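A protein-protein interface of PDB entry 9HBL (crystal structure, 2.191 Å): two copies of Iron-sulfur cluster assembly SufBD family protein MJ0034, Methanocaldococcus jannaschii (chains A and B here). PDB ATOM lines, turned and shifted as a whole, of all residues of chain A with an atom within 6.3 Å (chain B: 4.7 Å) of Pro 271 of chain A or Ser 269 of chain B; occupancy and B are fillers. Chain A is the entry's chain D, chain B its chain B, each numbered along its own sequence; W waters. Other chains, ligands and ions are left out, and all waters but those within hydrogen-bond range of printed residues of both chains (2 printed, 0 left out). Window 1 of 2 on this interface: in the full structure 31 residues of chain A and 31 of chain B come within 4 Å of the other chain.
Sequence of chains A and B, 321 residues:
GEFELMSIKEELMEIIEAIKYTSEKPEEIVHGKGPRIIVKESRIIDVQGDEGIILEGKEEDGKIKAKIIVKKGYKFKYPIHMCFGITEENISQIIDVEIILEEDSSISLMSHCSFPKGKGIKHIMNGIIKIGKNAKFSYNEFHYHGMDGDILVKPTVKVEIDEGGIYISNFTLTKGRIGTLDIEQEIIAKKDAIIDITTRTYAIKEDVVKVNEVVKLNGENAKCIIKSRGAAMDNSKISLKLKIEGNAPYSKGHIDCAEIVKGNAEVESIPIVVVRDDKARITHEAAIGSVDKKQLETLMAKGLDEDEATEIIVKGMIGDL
The backbone NH (N) of His 284 of chain A is in hydrogen-bond range of the backbone carbonyl oxygen (O) of Ala 286 of chain B (3.0 Å). O of Val 273 of chain A lies within hydrogen-bond range of N of Ser 269 of chain B (2.8 Å).
The backbone NH of Ile 270 of chain A lies within hydrogen-bond range of the backbone carbonyl oxygen of Leu 240 of chain A, 2.8 Å away. The backbone carbonyl oxygen (O) of Ile 270 of chain A lies within hydrogen-bond range of the backbone NH (N) of Leu 242 of chain A (3.1 Å). O of Leu 242 of chain A is in hydrogen-bond range of N of Ile 272 of chain A (2.9 Å). O of Glu 268 of chain B lies within hydrogen-bond range of N of Leu 240 of chain B. O of Leu 240 of chain B sits at hydrogen-bond distance from N of Ile 270 of chain B (2.8 Å).
Among the printed residues, pairs that only touch across the chains: Pro 271 of chain A with Pro 271 of chain B (3.1 Å), Val 274 of chain A with Val 267 of chain B (3.2 Å), Val 273 of chain A with Glu 268 of chain B (3.4 Å), Ile 272 of chain A with Ser 269 of chain B (3.4 Å), Val 273 of chain A with Val 267 of chain B (3.7 Å), Ile 270 of chain A with Ile 270 of chain B (3.7 Å), Val 273 of chain A with Ile 288 of chain B (3.7 Å), Ile 272 of chain A with Ile 270 of chain B (3.7 Å), Ser 269 of chain A with Pro 271 of chain B (3.8 Å) and Pro 271 of chain A with Ser 269 of chain B (3.8 Å).
Leu 242 of chain A touches none of the printed residues of chain B. Of the printed residues of chain B, Pro 271 of chain A touches Ser 269 (3.8 Å) and Pro 271 (3.1 Å). Of the printed residues of chain B, Val 273 of chain A touches Val 267 (3.7 Å), Glu 268 (3.4 Å), Ser 269 (2.8 Å) and Ile 288 (3.7 Å). Printed residues of chain B within 4 Å of Val 274 of chain A: Val 267 (3.2 Å). Printed residues of chain B within 4 Å of His 284 of chain A: Ala 286. Of the printed residues of chain A, Ser 269 of chain B touches Pro 271, Ile 272 and Val 273. The nearest printed residue of chain B that does not touch Pro 271 of chain A is Ile 270 of chain B (4.8 Å). The nearest printed residue of chain B that does not touch His 284 of chain A is Pro 271 of chain B (4.4 Å).
Printed residues of chain A that touch a printed residue of chain B: Ser 269, Ile 270, Pro 271, Ile 272, Val 273, Val 274 and His 284. Of the 9 printed residues of chain B, 7 touch a printed residue of chain A.
Ser 269 of chain A touches Pro 271 of chain B, and with the chains exchanged Pro 271 of chain A touches Ser 269 of chain B. Ile 270 of chain A touches its own counterpart, Ile 270 of chain B. Pro 271 of chain B touches its own counterpart, Pro 271 of chain A.
Water W2 bridges the side-chain amino group of Lys 243 of chain A and the side-chain carboxylate of Glu 268 of chain B. Water W1 lies within hydrogen-bond range of the side-chain carboxylate (OE1) of Glu 268 of chain B (3.0 Å) and the side-chain amino group (NZ) of Lys 243 of chain A (3.0 Å).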
ATOM      1  N   LEU A 240     -15.528  -4.883  24.014  1.00  0.00           N
ATOM      2  CA  LEU A 240     -16.777  -4.560  24.701  1.00  0.00           C
ATOM      3  C   LEU A 240     -16.993  -5.521  25.853  1.00  0.00           C
ATOM      4  O   LEU A 240     -17.362  -6.664  25.620  1.00  0.00           O
ATOM      5  CB  LEU A 240     -17.971  -4.657  23.739  1.00  0.00           C
ATOM      6  CG  LEU A 240     -17.798  -3.911  22.430  1.00  0.00           C
ATOM      7  CD1 LEU A 240     -18.668  -4.479  21.353  1.00  0.00           C
ATOM      8  CD2 LEU A 240     -17.986  -2.425  22.613  1.00  0.00           C
ATOM      9  N   LYS A 241     -16.779  -5.068  27.089  1.00  0.00           N
ATOM     10  CA  LYS A 241     -16.988  -5.875  28.276  1.00  0.00           C
ATOM     11  C   LYS A 241     -18.217  -5.304  28.961  1.00  0.00           C
ATOM     12  O   LYS A 241     -18.177  -4.180  29.429  1.00  0.00           O
ATOM     13  CB  LYS A 241     -15.747  -5.788  29.165  1.00  0.00           C
ATOM     14  CG  LYS A 241     -15.640  -6.947  30.135  1.00  0.00           C
ATOM     15  CD  LYS A 241     -14.533  -6.732  31.141  1.00  0.00           C
ATOM     16  CE  LYS A 241     -14.482  -7.882  32.106  1.00  0.00           C
ATOM     17  NZ  LYS A 241     -13.697  -7.549  33.330  1.00  0.00           N
ATOM     18  N   LEU A 242     -19.344  -6.017  28.923  1.00  0.00           N
ATOM     19  CA  LEU A 242     -20.630  -5.544  29.458  1.00  0.00           C
ATOM     20  C   LEU A 242     -21.095  -6.548  30.488  1.00  0.00           C
ATOM     21  O   LEU A 242     -21.152  -7.739  30.177  1.00  0.00           O
ATOM     22  CB  LEU A 242     -21.655  -5.481  28.329  1.00  0.00           C
ATOM     23  CG  LEU A 242     -21.230  -4.713  27.079  1.00  0.00           C
ATOM     24  CD1 LEU A 242     -22.251  -4.854  25.984  1.00  0.00           C
ATOM     25  CD2 LEU A 242     -20.963  -3.259  27.398  1.00  0.00           C
ATOM     26  N   LYS A 243     -21.440  -6.104  31.699  1.00  0.00           N
ATOM     27  CA  LYS A 243     -21.750  -7.034  32.786  1.00  0.00           C
ATOM     28  C   LYS A 243     -22.985  -6.713  33.578  1.00  0.00           C
ATOM     29  O   LYS A 243     -23.219  -5.554  33.903  1.00  0.00           O
ATOM     30  CB  LYS A 243     -20.534  -7.112  33.743  1.00  0.00           C
ATOM     31  CG  LYS A 243     -20.664  -8.076  34.916  1.00  0.00           C
ATOM     32  CD  LYS A 243     -19.389  -8.092  35.767  1.00  0.00           C
ATOM     33  CE  LYS A 243     -19.426  -9.174  36.820  1.00  0.00           C
ATOM     34  NZ  LYS A 243     -18.194  -9.200  37.670  1.00  0.00           N
ATOM     35  N   ILE A 255     -28.439  -8.110  28.004  1.00  0.00           N
ATOM     36  CA  ILE A 255     -27.294  -7.530  27.296  1.00  0.00           C
ATOM     37  C   ILE A 255     -27.508  -7.798  25.814  1.00  0.00           C
ATOM     38  O   ILE A 255     -27.755  -8.929  25.427  1.00  0.00           O
ATOM     39  CB  ILE A 255     -25.906  -8.080  27.772  1.00  0.00           C
ATOM     40  CG1 ILE A 255     -25.689  -7.932  29.302  1.00  0.00           C
ATOM     41  CG2 ILE A 255     -24.759  -7.401  26.989  1.00  0.00           C
ATOM     42  CD1 ILE A 255     -24.540  -8.788  29.827  1.00  0.00           C
ATOM     43  N   CYS A 257     -25.711  -7.065  22.127  1.00  0.00           N
ATOM     44  CA  CYS A 257     -24.508  -6.545  21.486  1.00  0.00           C
ATOM     45  C   CYS A 257     -24.480  -6.896  20.030  1.00  0.00           C
ATOM     46  O   CYS A 257     -24.742  -8.036  19.692  1.00  0.00           O
ATOM     47  CB  CYS A 257     -23.265  -7.059  22.206  1.00  0.00           C
ATOM     48  SG  CYS A 257     -21.739  -6.176  21.782  1.00  0.00           S
ATOM     49  N   SER A 269     -15.903  -9.350  22.223  1.00  0.00           N
ATOM     50  CA  SER A 269     -17.139  -9.125  22.951  1.00  0.00           C
ATOM     51  C   SER A 269     -17.172 -10.011  24.200  1.00  0.00           C
ATOM     52  O   SER A 269     -17.211 -11.237  24.092  1.00  0.00           O
ATOM     53  CB  SER A 269     -18.330  -9.401  22.041  1.00  0.00           C
ATOM     54  OG  SER A 269     -19.553  -9.294  22.748  1.00  0.00           O
ATOM     55  N   ILE A 270     -17.109  -9.403  25.385  1.00  0.00           N
ATOM     56  CA  ILE A 270     -17.106 -10.126  26.666  1.00  0.00           C
ATOM     57  C   ILE A 270     -18.308  -9.744  27.525  1.00  0.00           C
ATOM     58  O   ILE A 270     -18.225  -8.868  28.389  1.00  0.00           O
ATOM     59  CB  ILE A 270     -15.789  -9.978  27.468  1.00  0.00           C
ATOM     60  CG1 ILE A 270     -14.555 -10.056  26.553  1.00  0.00           C
ATOM     61  CG2 ILE A 270     -15.733 -11.018  28.582  1.00  0.00           C
ATOM     62  CD1 ILE A 270     -13.284  -9.699  27.211  1.00  0.00           C
ATOM     63  N   PRO A 271     -19.443 -10.418  27.316  1.00  0.00           N
ATOM     64  CA  PRO A 271     -20.654 -10.067  28.067  1.00  0.00           C
ATOM     65  C   PRO A 271     -20.900 -10.959  29.276  1.00  0.00           C
ATOM     66  O   PRO A 271     -21.501 -11.996  29.115  1.00  0.00           O
ATOM     67  CB  PRO A 271     -21.745 -10.235  27.024  1.00  0.00           C
ATOM     68  CG  PRO A 271     -21.173 -11.223  26.033  1.00  0.00           C
ATOM     69  CD  PRO A 271     -19.726 -11.443  26.301  1.00  0.00           C
ATOM     70  N   ILE A 272     -20.494 -10.542  30.465  1.00  0.00           N
ATOM     71  CA  ILE A 272     -20.620 -11.322  31.701  1.00  0.00           C
ATOM     72  C   ILE A 272     -21.993 -11.262  32.388  1.00  0.00           C
ATOM     73  O   ILE A 272     -22.540 -10.185  32.611  1.00  0.00           O
ATOM     74  CB  ILE A 272     -19.506 -10.879  32.685  1.00  0.00           C
ATOM     75  CG1 ILE A 272     -18.115 -11.038  32.046  1.00  0.00           C
ATOM     76  CG2 ILE A 272     -19.608 -11.637  33.999  1.00  0.00           C
ATOM     77  CD1 ILE A 272     -17.170 -10.147  32.502  1.00  0.00           C
ATOM     78  N   VAL A 273     -22.504 -12.426  32.797  1.00  0.00           N
ATOM     79  CA  VAL A 273     -23.754 -12.493  33.532  1.00  0.00           C
ATOM     80  C   VAL A 273     -23.529 -13.201  34.869  1.00  0.00           C
ATOM     81  O   VAL A 273     -23.084 -14.338  34.882  1.00  0.00           O
ATOM     82  CB  VAL A 273     -24.864 -13.158  32.688  1.00  0.00           C
ATOM     83  CG1 VAL A 273     -26.043 -13.591  33.555  1.00  0.00           C
ATOM     84  CG2 VAL A 273     -25.321 -12.228  31.562  1.00  0.00           C
ATOM     85  N   VAL A 274     -23.825 -12.533  35.986  1.00  0.00           N
ATOM     86  CA  VAL A 274     -23.685 -13.156  37.304  1.00  0.00           C
ATOM     87  C   VAL A 274     -25.055 -13.202  37.951  1.00  0.00           C
ATOM     88  O   VAL A 274     -25.738 -12.185  37.965  1.00  0.00           O
ATOM     89  CB  VAL A 274     -22.682 -12.422  38.233  1.00  0.00           C
ATOM     90  CG1 VAL A 274     -22.567 -13.129  39.564  1.00  0.00           C
ATOM     91  CG2 VAL A 274     -21.320 -12.281  37.577  1.00  0.00           C
ATOM     92  N   HIS A 284     -28.665 -12.629  27.594  1.00  0.00           N
ATOM     93  CA  HIS A 284     -27.778 -11.893  26.731  1.00  0.00           C
ATOM     94  C   HIS A 284     -27.894 -12.441  25.305  1.00  0.00           C
ATOM     95  O   HIS A 284     -28.260 -13.596  25.089  1.00  0.00           O
ATOM     96  CB  HIS A 284     -26.322 -11.870  27.290  1.00  0.00           C
ATOM     97  CG  HIS A 284     -25.277 -12.105  26.247  1.00  0.00           C
ATOM     98  ND1 HIS A 284     -24.782 -11.078  25.464  1.00  0.00           N
ATOM     99  CD2 HIS A 284     -24.829 -13.274  25.765  1.00  0.00           C
ATOM    100  CE1 HIS A 284     -24.013 -11.664  24.566  1.00  0.00           C
ATOM    101  NE2 HIS A 284     -23.999 -12.986  24.722  1.00  0.00           N
ATOM    102  N   ALA A 286     -25.738 -11.724  21.325  1.00  0.00           N
ATOM    103  CA  ALA A 286     -24.741 -10.957  20.595  1.00  0.00           C
ATOM    104  C   ALA A 286     -24.511 -11.509  19.219  1.00  0.00           C
ATOM    105  O   ALA A 286     -24.684 -12.706  18.986  1.00  0.00           O
ATOM    106  CB  ALA A 286     -23.437 -10.873  21.361  1.00  0.00           C
ATOM    107  N   LEU B 240     -18.792 -20.523  33.969  1.00  0.00           N
ATOM    108  CA  LEU B 240     -18.749 -21.020  32.596  1.00  0.00           C
ATOM    109  C   LEU B 240     -18.097 -19.995  31.682  1.00  0.00           C
ATOM    110  O   LEU B 240     -18.730 -18.999  31.345  1.00  0.00           O
ATOM    111  CB  LEU B 240     -20.170 -21.315  32.083  1.00  0.00           C
ATOM    112  CG  LEU B 240     -21.022 -22.173  33.003  1.00  0.00           C
ATOM    113  CD1 LEU B 240     -22.478 -21.964  32.776  1.00  0.00           C
ATOM    114  CD2 LEU B 240     -20.637 -23.611  32.927  1.00  0.00           C
ATOM    115  N   CYS B 257     -25.842 -20.886  26.120  1.00  0.00           N
ATOM    116  CA  CYS B 257     -25.683 -21.211  27.532  1.00  0.00           C
ATOM    117  C   CYS B 257     -26.978 -21.053  28.273  1.00  0.00           C
ATOM    118  O   CYS B 257     -27.645 -20.047  28.092  1.00  0.00           O
ATOM    119  CB  CYS B 257     -24.580 -20.352  28.141  1.00  0.00           C
ATOM    120  SG  CYS B 257     -24.005 -20.927  29.755  1.00  0.00           S
ATOM    121  N   VAL B 267     -24.000 -18.323  39.949  1.00  0.00           N
ATOM    122  CA  VAL B 267     -23.575 -18.620  38.599  1.00  0.00           C
ATOM    123  C   VAL B 267     -22.896 -17.433  37.938  1.00  0.00           C
ATOM    124  O   VAL B 267     -23.381 -16.307  37.999  1.00  0.00           O
ATOM    125  CB  VAL B 267     -24.791 -19.101  37.747  1.00  0.00           C
ATOM    126  CG1 VAL B 267     -24.397 -19.305  36.293  1.00  0.00           C
ATOM    127  CG2 VAL B 267     -25.401 -20.383  38.317  1.00  0.00           C
ATOM    128  N   GLU B 268     -21.827 -17.710  37.224  1.00  0.00           N
ATOM    129  CA  GLU B 268     -21.137 -16.725  36.426  1.00  0.00           C
ATOM    130  C   GLU B 268     -20.991 -17.262  34.990  1.00  0.00           C
ATOM    131  O   GLU B 268     -20.414 -18.328  34.774  1.00  0.00           O
ATOM    132  CB  GLU B 268     -19.797 -16.409  37.067  1.00  0.00           C
ATOM    133  CG  GLU B 268     -18.747 -15.874  36.136  1.00  0.00           C
ATOM    134  CD  GLU B 268     -17.495 -15.621  36.930  1.00  0.00           C
ATOM    135  OE1 GLU B 268     -17.410 -14.509  37.497  1.00  0.00           O
ATOM    136  OE2 GLU B 268     -16.641 -16.536  37.046  1.00  0.00           O
ATOM    137  N   SER B 269     -21.511 -16.524  34.022  1.00  0.00           N
ATOM    138  CA  SER B 269     -21.444 -16.913  32.621  1.00  0.00           C
ATOM    139  C   SER B 269     -20.603 -15.907  31.825  1.00  0.00           C
ATOM    140  O   SER B 269     -20.991 -14.748  31.694  1.00  0.00           O
ATOM    141  CB  SER B 269     -22.854 -17.024  32.055  1.00  0.00           C
ATOM    142  OG  SER B 269     -22.815 -17.334  30.675  1.00  0.00           O
ATOM    143  N   ILE B 270     -19.436 -16.330  31.339  1.00  0.00           N
ATOM    144  CA  ILE B 270     -18.520 -15.465  30.575  1.00  0.00           C
ATOM    145  C   ILE B 270     -18.292 -16.002  29.160  1.00  0.00           C
ATOM    146  O   ILE B 270     -17.332 -16.726  28.893  1.00  0.00           O
ATOM    147  CB  ILE B 270     -17.166 -15.200  31.282  1.00  0.00           C
ATOM    148  CG1 ILE B 270     -17.346 -14.969  32.787  1.00  0.00           C
ATOM    149  CG2 ILE B 270     -16.445 -14.033  30.606  1.00  0.00           C
ATOM    150  CD1 ILE B 270     -16.092 -14.947  33.543  1.00  0.00           C
ATOM    151  N   PRO B 271     -19.179 -15.640  28.230  1.00  0.00           N
ATOM    152  CA  PRO B 271     -19.050 -16.142  26.865  1.00  0.00           C
ATOM    153  C   PRO B 271     -18.351 -15.172  25.906  1.00  0.00           C
ATOM    154  O   PRO B 271     -19.020 -14.313  25.350  1.00  0.00           O
ATOM    155  CB  PRO B 271     -20.489 -16.343  26.475  1.00  0.00           C
ATOM    156  CG  PRO B 271     -21.275 -15.345  27.346  1.00  0.00           C
ATOM    157  CD  PRO B 271     -20.395 -14.827  28.394  1.00  0.00           C
ATOM    158  N   ALA B 286     -27.570 -16.490  25.951  1.00  0.00           N
ATOM    159  CA  ALA B 286     -27.526 -17.107  27.267  1.00  0.00           C
ATOM    160  C   ALA B 286     -28.685 -16.694  28.116  1.00  0.00           C
ATOM    161  O   ALA B 286     -29.198 -15.586  27.969  1.00  0.00           O
ATOM    162  CB  ALA B 286     -26.210 -16.812  27.973  1.00  0.00           C
ATOM    163  N   ILE B 288     -29.728 -17.092  32.253  1.00  0.00           N
ATOM    164  CA  ILE B 288     -29.175 -17.515  33.551  1.00  0.00           C
ATOM    165  C   ILE B 288     -30.100 -17.050  34.640  1.00  0.00           C
ATOM    166  O   ILE B 288     -30.565 -15.921  34.583  1.00  0.00           O
ATOM    167  CB  ILE B 288     -27.754 -16.879  33.751  1.00  0.00           C
ATOM    168  CG1 ILE B 288     -26.800 -17.168  32.563  1.00  0.00           C
ATOM    169  CG2 ILE B 288     -27.132 -17.265  35.098  1.00  0.00           C
ATOM    170  CD1 ILE B 288     -26.281 -18.580  32.447  1.00  0.00           C
HETATM  171  O   HOH W   1     -16.955 -11.737  36.518  1.00  0.00           O
HETATM  172  O   HOH W   2     -18.204 -11.657  39.146  1.00  0.00           O
